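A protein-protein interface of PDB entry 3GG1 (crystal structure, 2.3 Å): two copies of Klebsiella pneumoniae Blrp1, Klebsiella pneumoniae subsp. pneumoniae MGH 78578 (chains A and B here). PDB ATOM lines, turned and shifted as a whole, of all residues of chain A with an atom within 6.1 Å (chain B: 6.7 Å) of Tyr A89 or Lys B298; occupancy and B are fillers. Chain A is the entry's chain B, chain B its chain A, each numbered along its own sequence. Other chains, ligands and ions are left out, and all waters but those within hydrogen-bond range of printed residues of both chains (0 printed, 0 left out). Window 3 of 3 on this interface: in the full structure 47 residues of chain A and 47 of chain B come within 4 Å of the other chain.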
ATOM      1  N   MET A   9     -10.096  28.285  17.795  1.00  0.00           N
ATOM      2  CA  MET A   9     -11.453  28.916  17.777  1.00  0.00           C
ATOM      3  C   MET A   9     -12.460  28.058  18.530  1.00  0.00           C
ATOM      4  O   MET A   9     -12.490  26.842  18.358  1.00  0.00           O
ATOM      5  CB  MET A   9     -11.935  29.115  16.338  1.00  0.00           C
ATOM      6  CG  MET A   9     -11.127  30.130  15.550  1.00  0.00           C
ATOM      7  SD  MET A   9     -11.849  30.482  13.937  1.00  0.00           S
ATOM      8  CE  MET A   9     -11.498  28.982  13.035  1.00  0.00           C
ATOM      9  N   LEU A  10     -13.287  28.696  19.356  1.00  0.00           N
ATOM     10  CA  LEU A  10     -14.295  27.980  20.135  1.00  0.00           C
ATOM     11  C   LEU A  10     -15.285  27.275  19.207  1.00  0.00           C
ATOM     12  O   LEU A  10     -15.819  27.879  18.278  1.00  0.00           O
ATOM     13  CB  LEU A  10     -15.033  28.929  21.086  1.00  0.00           C
ATOM     14  CG  LEU A  10     -15.958  28.285  22.129  1.00  0.00           C
ATOM     15  CD1 LEU A  10     -15.215  27.244  22.963  1.00  0.00           C
ATOM     16  CD2 LEU A  10     -16.589  29.347  23.030  1.00  0.00           C
ATOM     17  N   THR A  11     -15.499  25.988  19.467  1.00  0.00           N
ATOM     18  CA  THR A  11     -16.358  25.133  18.656  1.00  0.00           C
ATOM     19  C   THR A  11     -17.351  24.418  19.571  1.00  0.00           C
ATOM     20  O   THR A  11     -17.067  24.184  20.750  1.00  0.00           O
ATOM     21  CB  THR A  11     -15.515  24.085  17.869  1.00  0.00           C
ATOM     22  OG1 THR A  11     -14.705  24.751  16.890  1.00  0.00           O
ATOM     23  CG2 THR A  11     -16.395  23.065  17.152  1.00  0.00           C
ATOM     24  N   THR A  12     -18.518  24.096  19.020  1.00  0.00           N
ATOM     25  CA  THR A  12     -19.511  23.271  19.693  1.00  0.00           C
ATOM     26  C   THR A  12     -19.639  21.947  18.941  1.00  0.00           C
ATOM     27  O   THR A  12     -19.601  21.918  17.713  1.00  0.00           O
ATOM     28  CB  THR A  12     -20.882  23.979  19.740  1.00  0.00           C
ATOM     29  OG1 THR A  12     -20.793  25.136  20.584  1.00  0.00           O
ATOM     30  CG2 THR A  12     -21.968  23.048  20.279  1.00  0.00           C
ATOM     31  N   GLU A  63     -11.581  23.691  18.124  1.00  0.00           N
ATOM     32  CA  GLU A  63     -11.883  22.757  17.040  1.00  0.00           C
ATOM     33  C   GLU A  63     -11.004  21.513  17.133  1.00  0.00           C
ATOM     34  O   GLU A  63     -11.495  20.384  17.059  1.00  0.00           O
ATOM     35  CB  GLU A  63     -11.669  23.446  15.687  1.00  0.00           C
ATOM     36  CG  GLU A  63     -12.149  22.653  14.475  1.00  0.00           C
ATOM     37  CD  GLU A  63     -12.059  23.455  13.182  1.00  0.00           C
ATOM     38  OE1 GLU A  63     -11.053  24.170  12.987  1.00  0.00           O
ATOM     39  OE2 GLU A  63     -12.996  23.365  12.358  1.00  0.00           O
ATOM     40  N   MET A  86     -24.715  18.262  15.778  1.00  0.00           N
ATOM     41  CA  MET A  86     -24.304  19.645  15.572  1.00  0.00           C
ATOM     42  C   MET A  86     -22.791  19.789  15.641  1.00  0.00           C
ATOM     43  O   MET A  86     -22.126  19.129  16.440  1.00  0.00           O
ATOM     44  CB  MET A  86     -24.949  20.545  16.625  1.00  0.00           C
ATOM     45  CG  MET A  86     -24.557  22.011  16.532  1.00  0.00           C
ATOM     46  SD  MET A  86     -25.539  23.040  17.631  1.00  0.00           S
ATOM     47  CE  MET A  86     -24.783  24.640  17.350  1.00  0.00           C
ATOM     48  N   ARG A  87     -22.261  20.669  14.798  1.00  0.00           N
ATOM     49  CA  ARG A  87     -20.840  20.979  14.783  1.00  0.00           C
ATOM     50  C   ARG A  87     -20.665  22.366  14.187  1.00  0.00           C
ATOM     51  O   ARG A  87     -20.834  22.552  12.982  1.00  0.00           O
ATOM     52  CB  ARG A  87     -20.079  19.935  13.969  1.00  0.00           C
ATOM     53  CG  ARG A  87     -18.581  19.919  14.195  1.00  0.00           C
ATOM     54  CD  ARG A  87     -17.960  18.720  13.488  1.00  0.00           C
ATOM     55  NE  ARG A  87     -16.716  18.271  14.109  1.00  0.00           N
ATOM     56  CZ  ARG A  87     -16.231  17.032  14.033  1.00  0.00           C
ATOM     57  NH1 ARG A  87     -16.884  16.077  13.377  1.00  0.00           N
ATOM     58  NH2 ARG A  87     -15.085  16.737  14.630  1.00  0.00           N
ATOM     59  N   ASP A  88     -20.360  23.342  15.038  1.00  0.00           N
ATOM     60  CA  ASP A  88     -20.258  24.735  14.609  1.00  0.00           C
ATOM     61  C   ASP A  88     -19.343  25.562  15.498  1.00  0.00           C
ATOM     62  O   ASP A  88     -19.092  25.212  16.651  1.00  0.00           O
ATOM     63  CB  ASP A  88     -21.649  25.380  14.593  1.00  0.00           C
ATOM     64  CG  ASP A  88     -22.186  25.583  13.193  1.00  0.00           C
ATOM     65  OD1 ASP A  88     -21.425  26.058  12.319  1.00  0.00           O
ATOM     66  OD2 ASP A  88     -23.377  25.285  12.976  1.00  0.00           O
ATOM     67  N   TYR A  89     -18.856  26.668  14.947  1.00  0.00           N
ATOM     68  CA  TYR A  89     -18.097  27.641  15.718  1.00  0.00           C
ATOM     69  C   TYR A  89     -19.045  28.363  16.664  1.00  0.00           C
ATOM     70  O   TYR A  89     -20.234  28.510  16.372  1.00  0.00           O
ATOM     71  CB  TYR A  89     -17.386  28.640  14.800  1.00  0.00           C
ATOM     72  CG  TYR A  89     -16.358  27.993  13.901  1.00  0.00           C
ATOM     73  CD1 TYR A  89     -15.124  27.594  14.404  1.00  0.00           C
ATOM     74  CD2 TYR A  89     -16.626  27.766  12.554  1.00  0.00           C
ATOM     75  CE1 TYR A  89     -14.178  26.992  13.590  1.00  0.00           C
ATOM     76  CE2 TYR A  89     -15.686  27.165  11.727  1.00  0.00           C
ATOM     77  CZ  TYR A  89     -14.462  26.778  12.253  1.00  0.00           C
ATOM     78  OH  TYR A  89     -13.521  26.181  11.446  1.00  0.00           O
ATOM     79  N   SER A  90     -18.507  28.813  17.790  1.00  0.00           N
ATOM     80  CA  SER A  90     -19.312  29.351  18.877  1.00  0.00           C
ATOM     81  C   SER A  90     -18.736  30.671  19.381  1.00  0.00           C
ATOM     82  O   SER A  90     -17.521  30.884  19.346  1.00  0.00           O
ATOM     83  CB  SER A  90     -19.379  28.329  20.014  1.00  0.00           C
ATOM     84  OG  SER A  90     -19.969  28.882  21.173  1.00  0.00           O
ATOM     85  N   ALA A  91     -19.619  31.550  19.850  1.00  0.00           N
ATOM     86  CA  ALA A  91     -19.230  32.880  20.328  1.00  0.00           C
ATOM     87  C   ALA A  91     -18.907  32.897  21.821  1.00  0.00           C
ATOM     88  O   ALA A  91     -18.191  33.778  22.289  1.00  0.00           O
ATOM     89  CB  ALA A  91     -20.329  33.879  20.027  1.00  0.00           C
ATOM     90  N   PHE B 293     -20.640  32.778   0.788  1.00  0.00           N
ATOM     91  CA  PHE B 293     -21.555  32.774   1.934  1.00  0.00           C
ATOM     92  C   PHE B 293     -20.989  32.091   3.184  1.00  0.00           C
ATOM     93  O   PHE B 293     -21.203  32.571   4.297  1.00  0.00           O
ATOM     94  CB  PHE B 293     -22.889  32.114   1.554  1.00  0.00           C
ATOM     95  CG  PHE B 293     -23.923  32.172   2.643  1.00  0.00           C
ATOM     96  CD1 PHE B 293     -24.130  31.084   3.484  1.00  0.00           C
ATOM     97  CD2 PHE B 293     -24.680  33.322   2.839  1.00  0.00           C
ATOM     98  CE1 PHE B 293     -25.077  31.138   4.495  1.00  0.00           C
ATOM     99  CE2 PHE B 293     -25.630  33.383   3.847  1.00  0.00           C
ATOM    100  CZ  PHE B 293     -25.830  32.289   4.676  1.00  0.00           C
ATOM    101  N   ARG B 294     -20.283  30.979   2.992  1.00  0.00           N
ATOM    102  CA  ARG B 294     -19.731  30.196   4.104  1.00  0.00           C
ATOM    103  C   ARG B 294     -18.768  31.007   4.967  1.00  0.00           C
ATOM    104  O   ARG B 294     -18.766  30.880   6.193  1.00  0.00           O
ATOM    105  CB  ARG B 294     -19.002  28.956   3.581  1.00  0.00           C
ATOM    106  CG  ARG B 294     -19.901  27.909   2.941  1.00  0.00           C
ATOM    107  CD  ARG B 294     -19.071  26.872   2.186  1.00  0.00           C
ATOM    108  NE  ARG B 294     -18.122  26.190   3.068  1.00  0.00           N
ATOM    109  CZ  ARG B 294     -17.052  25.504   2.659  1.00  0.00           C
ATOM    110  NH1 ARG B 294     -16.758  25.392   1.364  1.00  0.00           N
ATOM    111  NH2 ARG B 294     -16.260  24.925   3.561  1.00  0.00           N
ATOM    112  N   LYS B 295     -17.951  31.833   4.319  1.00  0.00           N
ATOM    113  CA  LYS B 295     -16.998  32.695   5.019  1.00  0.00           C
ATOM    114  C   LYS B 295     -17.755  33.730   5.857  1.00  0.00           C
ATOM    115  O   LYS B 295     -17.366  34.036   6.986  1.00  0.00           O
ATOM    116  CB  LYS B 295     -16.071  33.412   4.023  1.00  0.00           C
ATOM    117  CG  LYS B 295     -14.606  33.495   4.454  1.00  0.00           C
ATOM    118  CD  LYS B 295     -13.751  32.470   3.707  1.00  0.00           C
ATOM    119  CE  LYS B 295     -12.338  32.368   4.271  1.00  0.00           C
ATOM    120  NZ  LYS B 295     -11.579  33.646   4.152  1.00  0.00           N
ATOM    121  N   VAL B 296     -18.830  34.266   5.283  1.00  0.00           N
ATOM    122  CA  VAL B 296     -19.679  35.237   5.967  1.00  0.00           C
ATOM    123  C   VAL B 296     -20.430  34.563   7.112  1.00  0.00           C
ATOM    124  O   VAL B 296     -20.501  35.109   8.213  1.00  0.00           O
ATOM    125  CB  VAL B 296     -20.680  35.905   4.986  1.00  0.00           C
ATOM    126  CG1 VAL B 296     -21.707  36.751   5.733  1.00  0.00           C
ATOM    127  CG2 VAL B 296     -19.930  36.755   3.969  1.00  0.00           C
ATOM    128  N   LEU B 297     -20.979  33.380   6.853  1.00  0.00           N
ATOM    129  CA  LEU B 297     -21.680  32.617   7.889  1.00  0.00           C
ATOM    130  C   LEU B 297     -20.747  32.258   9.048  1.00  0.00           C
ATOM    131  O   LEU B 297     -21.123  32.369  10.216  1.00  0.00           O
ATOM    132  CB  LEU B 297     -22.304  31.346   7.300  1.00  0.00           C
ATOM    133  CG  LEU B 297     -22.965  30.374   8.288  1.00  0.00           C
ATOM    134  CD1 LEU B 297     -23.882  31.080   9.282  1.00  0.00           C
ATOM    135  CD2 LEU B 297     -23.744  29.318   7.532  1.00  0.00           C
ATOM    136  N   LYS B 298     -19.533  31.832   8.714  1.00  0.00           N
ATOM    137  CA  LYS B 298     -18.519  31.537   9.718  1.00  0.00           C
ATOM    138  C   LYS B 298     -18.297  32.737  10.645  1.00  0.00           C
ATOM    139  O   LYS B 298     -18.299  32.589  11.862  1.00  0.00           O
ATOM    140  CB  LYS B 298     -17.203  31.136   9.044  1.00  0.00           C
ATOM    141  CG  LYS B 298     -16.117  30.705  10.014  1.00  0.00           C
ATOM    142  CD  LYS B 298     -14.819  30.391   9.289  1.00  0.00           C
ATOM    143  CE  LYS B 298     -13.714  30.001  10.267  1.00  0.00           C
ATOM    144  NZ  LYS B 298     -13.468  31.051  11.300  1.00  0.00           N
ATOM    145  N   ALA B 299     -18.121  33.919  10.058  1.00  0.00           N
ATOM    146  CA  ALA B 299     -17.912  35.147  10.830  1.00  0.00           C
ATOM    147  C   ALA B 299     -19.110  35.496  11.719  1.00  0.00           C
ATOM    148  O   ALA B 299     -18.931  35.917  12.861  1.00  0.00           O
ATOM    149  CB  ALA B 299     -17.587  36.311   9.902  1.00  0.00           C
ATOM    150  N   LEU B 300     -20.322  35.321  11.197  1.00  0.00           N
ATOM    151  CA  LEU B 300     -21.542  35.569  11.975  1.00  0.00           C
ATOM    152  C   LEU B 300     -21.594  34.686  13.222  1.00  0.00           C
ATOM    153  O   LEU B 300     -21.865  35.172  14.323  1.00  0.00           O
ATOM    154  CB  LEU B 300     -22.796  35.328  11.125  1.00  0.00           C
ATOM    155  CG  LEU B 300     -23.085  36.315   9.991  1.00  0.00           C
ATOM    156  CD1 LEU B 300     -24.239  35.827   9.121  1.00  0.00           C
ATOM    157  CD2 LEU B 300     -23.381  37.692  10.539  1.00  0.00           C
ATOM    158  N   ARG B 301     -21.327  33.392  13.035  1.00  0.00           N
ATOM    159  CA  ARG B 301     -21.326  32.416  14.131  1.00  0.00           C
ATOM    160  C   ARG B 301     -20.261  32.717  15.184  1.00  0.00           C
ATOM    161  O   ARG B 301     -20.523  32.613  16.383  1.00  0.00           O
ATOM    162  CB  ARG B 301     -21.110  31.000  13.585  1.00  0.00           C
ATOM    163  CG  ARG B 301     -22.316  30.438  12.849  1.00  0.00           C
ATOM    164  CD  ARG B 301     -23.324  29.830  13.810  1.00  0.00           C
ATOM    165  NE  ARG B 301     -24.688  29.897  13.289  1.00  0.00           N
ATOM    166  CZ  ARG B 301     -25.195  29.095  12.353  1.00  0.00           C
ATOM    167  NH1 ARG B 301     -24.460  28.132  11.794  1.00  0.00           N
ATOM    168  NH2 ARG B 301     -26.455  29.262  11.968  1.00  0.00           N
ATOM    169  N   VAL B 302     -19.065  33.083  14.729  1.00  0.00           N
ATOM    170  CA  VAL B 302     -17.959  33.419  15.629  1.00  0.00           C
ATOM    171  C   VAL B 302     -18.279  34.691  16.420  1.00  0.00           C
ATOM    172  O   VAL B 302     -17.977  34.778  17.610  1.00  0.00           O
ATOM    173  CB  VAL B 302     -16.624  33.597  14.853  1.00  0.00           C
ATOM    174  CG1 VAL B 302     -15.521  34.091  15.776  1.00  0.00           C
ATOM    175  CG2 VAL B 302     -16.204  32.282  14.185  1.00  0.00           C
ATOM    176  N   ALA B 303     -18.896  35.665  15.753  1.00  0.00           N
ATOM    177  CA  ALA B 303     -19.316  36.909  16.400  1.00  0.00           C
ATOM    178  C   ALA B 303     -20.521  36.712  17.328  1.00  0.00           C
ATOM    179  O   ALA B 303     -20.722  37.496  18.255  1.00  0.00           O
ATOM    180  CB  ALA B 303     -19.625  37.968  15.356  1.00  0.00           C
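Glu A63 touches none of the printed residues of chain B. Of the printed residues of chain B, Asp A88 touches Arg B301 (3.3 Å). Of chain B, only Lys B298 (3.8 Å), Arg B301 (3.8 Å) and Val B302 (3.9 Å) come within 4 Å of Tyr A89. Of the printed residues of chain B, Ser A90 touches Arg B301. Of the printed residues of chain B, Ala A91 touches Arg B301, Val B302 and Ala B303. Of chain A, only Met A9 and Tyr A89 come within 4 Å of Lys B298. Printed residues of chain A within 4 Å of Arg B301: Asp A88, Tyr A89, Ser A90 and Ala A91. Printed residues of chain A within 4 Å of Val B302: Tyr A89 and Ala A91. The nearest printed residue of chain B that does not touch Tyr A89 is Ala B299 (6.8 Å). The nearest printed residue of chain A that does not touch Lys B298 is Asp A88 (6.7 Å). The nearest printed residue of chain B that does not touch Ala A91 is Leu B300 (6.0 Å).
The backbone carbonyl oxygen (O) of Met A9 sits at hydrogen-bond distance from the side-chain hydroxyl (OG1) of Thr A11, at 3.4 Å. O of Met A9 lies within hydrogen-bond range of N of Glu A63 (3.3 Å). The backbone carbonyl oxygen (O) of Leu A10 lies within hydrogen-bond range of the backbone NH (N) of Ser A90 (2.9 Å). O of Asp A88 is in hydrogen-bond range of N of Thr A12. The side-chain carboxylate (OE2) of Glu A63 sits at hydrogen-bond distance from the side-chain hydroxyl (OH) of Tyr A89 (3.0 Å).
The side-chain amino group of Lys B298 lies within hydrogen-bond range of the side-chain sulfur of Met A9 (3.1 Å). OD2 of Asp A88 lies within salt-bridge range of NH1 of Arg B301 (3.3 Å).
Of the 11 printed residues of chain B, 4 touch a printed residue of chain A. Of the 11 printed residues of chain A, 5 touch a printed residue of chain B.
No position is printed for both chains. Of the 9 pairs that touch across the chains among the printed residues, none has its exchanged pair printed and touching as well.
Among the printed residues, merely in contact across the chains: Tyr A89 with Lys B298, Tyr A89 with Arg B301, Tyr A89 with Val B302, Ser A90 with Arg B301, Ala A91 with Arg B301, Ala A91 with Val B302 and Ala A91 with Ala B303.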
